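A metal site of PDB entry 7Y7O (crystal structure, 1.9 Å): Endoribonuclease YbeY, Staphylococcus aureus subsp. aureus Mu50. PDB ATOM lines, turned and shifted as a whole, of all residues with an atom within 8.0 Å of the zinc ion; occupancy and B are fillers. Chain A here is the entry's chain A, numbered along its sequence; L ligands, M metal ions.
The backbone carbonyl oxygen (O) of Tyr 129 sits at hydrogen-bond distance from a ring nitrogen (ND1) of His 125 (3.2 Å).
OE1 of Gln 144 is in hydrogen-bond range of ND1 of His 121 (2.7 Å).
The zinc ion is bound by O2 of the ligand, O3 of the ligand, O6 of the ligand, NE2 of His 125, NE2 of His 121 and NE2 of His 131.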
ATOM      1  N   ARG A  59     -10.936  -8.025   8.539  1.00  0.00           N
ATOM      2  CA  ARG A  59      -9.634  -7.571   8.992  1.00  0.00           C
ATOM      3  C   ARG A  59      -9.253  -8.161  10.342  1.00  0.00           C
ATOM      4  O   ARG A  59      -8.170  -7.848  10.853  1.00  0.00           O
ATOM      5  CB  ARG A  59      -9.615  -6.031   9.068  1.00  0.00           C
ATOM      6  CG  ARG A  59      -9.665  -5.302   7.708  1.00  0.00           C
ATOM      7  CD  ARG A  59      -8.252  -5.099   7.165  1.00  0.00           C
ATOM      8  NE  ARG A  59      -8.181  -4.401   5.883  1.00  0.00           N
ATOM      9  CZ  ARG A  59      -8.044  -3.085   5.720  1.00  0.00           C
ATOM     10  NH1 ARG A  59      -8.101  -2.234   6.742  1.00  0.00           N
ATOM     11  NH2 ARG A  59      -7.804  -2.609   4.495  1.00  0.00           N
ATOM     12  N   ASP A  66     -12.704   4.457  10.913  1.00  0.00           N
ATOM     13  CA  ASP A  66     -13.292   5.476  10.041  1.00  0.00           C
ATOM     14  C   ASP A  66     -13.367   5.044   8.578  1.00  0.00           C
ATOM     15  O   ASP A  66     -14.365   5.333   7.904  1.00  0.00           O
ATOM     16  CB  ASP A  66     -12.519   6.800  10.134  1.00  0.00           C
ATOM     17  CG  ASP A  66     -11.010   6.636   9.991  1.00  0.00           C
ATOM     18  OD1 ASP A  66     -10.469   5.502   9.892  1.00  0.00           O
ATOM     19  OD2 ASP A  66     -10.359   7.709   9.967  1.00  0.00           O
ATOM     20  N   VAL A  67     -12.328   4.370   8.067  1.00  0.00           N
ATOM     21  CA  VAL A  67     -12.276   3.988   6.652  1.00  0.00           C
ATOM     22  C   VAL A  67     -11.539   2.653   6.540  1.00  0.00           C
ATOM     23  O   VAL A  67     -10.578   2.388   7.270  1.00  0.00           O
ATOM     24  CB  VAL A  67     -11.608   5.083   5.791  1.00  0.00           C
ATOM     25  CG1 VAL A  67     -10.157   5.313   6.191  1.00  0.00           C
ATOM     26  CG2 VAL A  67     -11.693   4.749   4.296  1.00  0.00           C
ATOM     27  N   SER A  69     -10.071   0.210   3.214  1.00  0.00           N
ATOM     28  CA  SER A  69      -9.877   0.118   1.779  1.00  0.00           C
ATOM     29  C   SER A  69      -9.523  -1.321   1.400  1.00  0.00           C
ATOM     30  O   SER A  69      -8.728  -1.963   2.079  1.00  0.00           O
ATOM     31  CB  SER A  69      -8.792   1.071   1.305  1.00  0.00           C
ATOM     32  OG  SER A  69      -7.526   0.710   1.822  1.00  0.00           O
ATOM     33  N   LEU A 118     -11.602  11.134   3.723  1.00  0.00           N
ATOM     34  CA  LEU A 118     -11.430   9.693   3.923  1.00  0.00           C
ATOM     35  C   LEU A 118     -11.503   8.951   2.595  1.00  0.00           C
ATOM     36  O   LEU A 118     -10.765   7.993   2.378  1.00  0.00           O
ATOM     37  CB  LEU A 118     -12.491   9.163   4.883  1.00  0.00           C
ATOM     38  CG  LEU A 118     -12.345   9.722   6.311  1.00  0.00           C
ATOM     39  CD1 LEU A 118     -13.570   9.357   7.156  1.00  0.00           C
ATOM     40  CD2 LEU A 118     -11.048   9.179   6.932  1.00  0.00           C
ATOM     41  N   HIS A 121      -8.163   9.461   0.924  1.00  0.00           N
ATOM     42  CA  HIS A 121      -7.167   8.611   1.576  1.00  0.00           C
ATOM     43  C   HIS A 121      -7.295   7.167   1.098  1.00  0.00           C
ATOM     44  O   HIS A 121      -6.292   6.528   0.747  1.00  0.00           O
ATOM     45  CB  HIS A 121      -7.351   8.692   3.081  1.00  0.00           C
ATOM     46  CG  HIS A 121      -6.263   7.996   3.831  1.00  0.00           C
ATOM     47  ND1 HIS A 121      -4.965   8.464   3.829  1.00  0.00           N
ATOM     48  CD2 HIS A 121      -6.257   6.841   4.541  1.00  0.00           C
ATOM     49  CE1 HIS A 121      -4.205   7.638   4.537  1.00  0.00           C
ATOM     50  NE2 HIS A 121      -4.977   6.656   4.982  1.00  0.00           N
ATOM     51  N   GLY A 122      -8.519   6.636   1.079  1.00  0.00           N
ATOM     52  CA  GLY A 122      -8.719   5.280   0.590  1.00  0.00           C
ATOM     53  C   GLY A 122      -8.329   5.115  -0.865  1.00  0.00           C
ATOM     54  O   GLY A 122      -7.739   4.110  -1.249  1.00  0.00           O
ATOM     55  N   LEU A 124      -6.011   6.713  -2.521  1.00  0.00           N
ATOM     56  CA  LEU A 124      -4.563   6.618  -2.640  1.00  0.00           C
ATOM     57  C   LEU A 124      -4.065   5.244  -2.197  1.00  0.00           C
ATOM     58  O   LEU A 124      -3.119   4.700  -2.777  1.00  0.00           O
ATOM     59  CB  LEU A 124      -3.918   7.728  -1.814  1.00  0.00           C
ATOM     60  CG  LEU A 124      -4.131   9.148  -2.383  1.00  0.00           C
ATOM     61  CD1 LEU A 124      -3.465  10.170  -1.476  1.00  0.00           C
ATOM     62  CD2 LEU A 124      -3.569   9.275  -3.805  1.00  0.00           C
ATOM     63  N   HIS A 125      -4.708   4.664  -1.173  1.00  0.00           N
ATOM     64  CA  HIS A 125      -4.393   3.282  -0.800  1.00  0.00           C
ATOM     65  C   HIS A 125      -4.634   2.319  -1.955  1.00  0.00           C
ATOM     66  O   HIS A 125      -3.835   1.404  -2.189  1.00  0.00           O
ATOM     67  CB  HIS A 125      -5.242   2.872   0.399  1.00  0.00           C
ATOM     68  CG  HIS A 125      -4.584   3.151   1.708  1.00  0.00           C
ATOM     69  ND1 HIS A 125      -3.380   2.595   2.064  1.00  0.00           N
ATOM     70  CD2 HIS A 125      -4.958   3.952   2.736  1.00  0.00           C
ATOM     71  CE1 HIS A 125      -3.035   3.033   3.263  1.00  0.00           C
ATOM     72  NE2 HIS A 125      -3.973   3.855   3.693  1.00  0.00           N
ATOM     73  N   TYR A 129      -0.334   3.323  -2.611  1.00  0.00           N
ATOM     74  CA  TYR A 129       0.389   4.056  -1.584  1.00  0.00           C
ATOM     75  C   TYR A 129       0.113   3.441  -0.222  1.00  0.00           C
ATOM     76  O   TYR A 129      -0.935   2.825  -0.003  1.00  0.00           O
ATOM     77  CB  TYR A 129      -0.029   5.532  -1.558  1.00  0.00           C
ATOM     78  CG  TYR A 129       0.349   6.323  -2.803  1.00  0.00           C
ATOM     79  CD1 TYR A 129       1.608   6.910  -2.914  1.00  0.00           C
ATOM     80  CD2 TYR A 129      -0.567   6.531  -3.835  1.00  0.00           C
ATOM     81  CE1 TYR A 129       1.950   7.650  -4.037  1.00  0.00           C
ATOM     82  CE2 TYR A 129      -0.237   7.265  -4.961  1.00  0.00           C
ATOM     83  CZ  TYR A 129       1.030   7.827  -5.050  1.00  0.00           C
ATOM     84  OH  TYR A 129       1.374   8.559  -6.155  1.00  0.00           O
ATOM     85  N   ASP A 130       1.043   3.617   0.708  1.00  0.00           N
ATOM     86  CA  ASP A 130       0.812   3.232   2.084  1.00  0.00           C
ATOM     87  C   ASP A 130       1.617   4.144   2.999  1.00  0.00           C
ATOM     88  O   ASP A 130       2.390   4.986   2.535  1.00  0.00           O
ATOM     89  CB  ASP A 130       1.152   1.759   2.326  1.00  0.00           C
ATOM     90  CG  ASP A 130       0.283   1.119   3.413  1.00  0.00           C
ATOM     91  OD1 ASP A 130      -0.260   1.824   4.296  1.00  0.00           O
ATOM     92  OD2 ASP A 130       0.162  -0.131   3.384  1.00  0.00           O
ATOM     93  N   HIS A 131       1.406   3.990   4.302  1.00  0.00           N
ATOM     94  CA  HIS A 131       2.062   4.866   5.265  1.00  0.00           C
ATOM     95  C   HIS A 131       2.454   4.080   6.504  1.00  0.00           C
ATOM     96  O   HIS A 131       2.361   4.577   7.632  1.00  0.00           O
ATOM     97  CB  HIS A 131       1.186   6.054   5.647  1.00  0.00           C
ATOM     98  CG  HIS A 131      -0.192   5.666   6.084  1.00  0.00           C
ATOM     99  ND1 HIS A 131      -0.538   5.508   7.403  1.00  0.00           N
ATOM    100  CD2 HIS A 131      -1.311   5.436   5.359  1.00  0.00           C
ATOM    101  CE1 HIS A 131      -1.815   5.179   7.488  1.00  0.00           C
ATOM    102  NE2 HIS A 131      -2.307   5.136   6.265  1.00  0.00           N
ATOM    103  N   MET A 132       2.899   2.849   6.312  1.00  0.00           N
ATOM    104  CA  MET A 132       3.310   2.041   7.453  1.00  0.00           C
ATOM    105  C   MET A 132       4.775   2.240   7.805  1.00  0.00           C
ATOM    106  O   MET A 132       5.182   1.891   8.921  1.00  0.00           O
ATOM    107  CB  MET A 132       3.029   0.572   7.159  1.00  0.00           C
ATOM    108  CG  MET A 132       1.535   0.317   7.091  1.00  0.00           C
ATOM    109  SD  MET A 132       1.220  -1.398   7.347  1.00  0.00           S
ATOM    110  CE  MET A 132       1.388  -1.304   9.092  1.00  0.00           C
ATOM    111  N   MET A 140       3.289   9.193   0.613  1.00  0.00           N
ATOM    112  CA  MET A 140       1.842   9.148   0.417  1.00  0.00           C
ATOM    113  C   MET A 140       1.193  10.429   0.928  1.00  0.00           C
ATOM    114  O   MET A 140       0.357  11.015   0.226  1.00  0.00           O
ATOM    115  CB  MET A 140       1.247   7.928   1.108  1.00  0.00           C
ATOM    116  CG  MET A 140      -0.274   7.979   1.178  1.00  0.00           C
ATOM    117  SD  MET A 140      -0.982   6.538   1.996  1.00  0.00           S
ATOM    118  CE  MET A 140      -2.698   6.601   1.424  1.00  0.00           C
ATOM    119  N   PHE A 141       1.551  10.869   2.138  1.00  0.00           N
ATOM    120  CA  PHE A 141       1.008  12.145   2.598  1.00  0.00           C
ATOM    121  C   PHE A 141       1.513  13.319   1.770  1.00  0.00           C
ATOM    122  O   PHE A 141       0.820  14.343   1.663  1.00  0.00           O
ATOM    123  CB  PHE A 141       1.268  12.400   4.081  1.00  0.00           C
ATOM    124  CG  PHE A 141       0.710  11.354   5.002  1.00  0.00           C
ATOM    125  CD1 PHE A 141      -0.122  10.361   4.534  1.00  0.00           C
ATOM    126  CD2 PHE A 141       0.900  11.465   6.369  1.00  0.00           C
ATOM    127  CE1 PHE A 141      -0.673   9.420   5.392  1.00  0.00           C
ATOM    128  CE2 PHE A 141       0.345  10.544   7.236  1.00  0.00           C
ATOM    129  CZ  PHE A 141      -0.449   9.516   6.740  1.00  0.00           C
ATOM    130  N   GLN A 144      -1.008  13.294  -0.939  1.00  0.00           N
ATOM    131  CA  GLN A 144      -2.284  13.719  -0.373  1.00  0.00           C
ATOM    132  C   GLN A 144      -2.311  15.227  -0.156  1.00  0.00           C
ATOM    133  O   GLN A 144      -3.285  15.902  -0.525  1.00  0.00           O
ATOM    134  CB  GLN A 144      -2.495  12.983   0.953  1.00  0.00           C
ATOM    135  CG  GLN A 144      -3.900  12.773   1.373  1.00  0.00           C
ATOM    136  CD  GLN A 144      -3.953  11.797   2.540  1.00  0.00           C
ATOM    137  OE1 GLN A 144      -4.240  10.616   2.354  1.00  0.00           O
ATOM    138  NE2 GLN A 144      -3.632  12.277   3.715  1.00  0.00           N
HETATM  139  C1  LIG L   1      -5.828   4.798   8.429  1.00  0.00           C
HETATM  140  O1  LIG L   1      -5.891   5.333   9.551  1.00  0.00           O
HETATM  141  O2  LIG L   1      -4.956   5.186   7.635  1.00  0.00           O
HETATM  142  C2  LIG L   1      -6.831   3.729   8.068  1.00  0.00           C
HETATM  143  C3  LIG L   1      -6.440   2.931   6.833  1.00  0.00           C
HETATM  144  O3  LIG L   1      -6.391   3.815   5.669  1.00  0.00           O
HETATM  145  C4  LIG L   1      -7.489   1.842   6.663  1.00  0.00           C
HETATM  146  C5  LIG L   1      -7.418   1.135   5.321  1.00  0.00           C
HETATM  147  O4  LIG L   1      -6.929   1.707   4.334  1.00  0.00           O
HETATM  148  O5  LIG L   1      -7.849  -0.032   5.193  1.00  0.00           O
HETATM  149  C6  LIG L   1      -5.102   2.252   7.072  1.00  0.00           C
HETATM  150  O6  LIG L   1      -4.055   2.629   6.505  1.00  0.00           O
HETATM  151  O7  LIG L   1      -5.037   1.292   7.866  1.00  0.00           O
HETATM  152 ZN    ZN M   1      -4.416   4.642   5.716  1.00  0.00          ZN
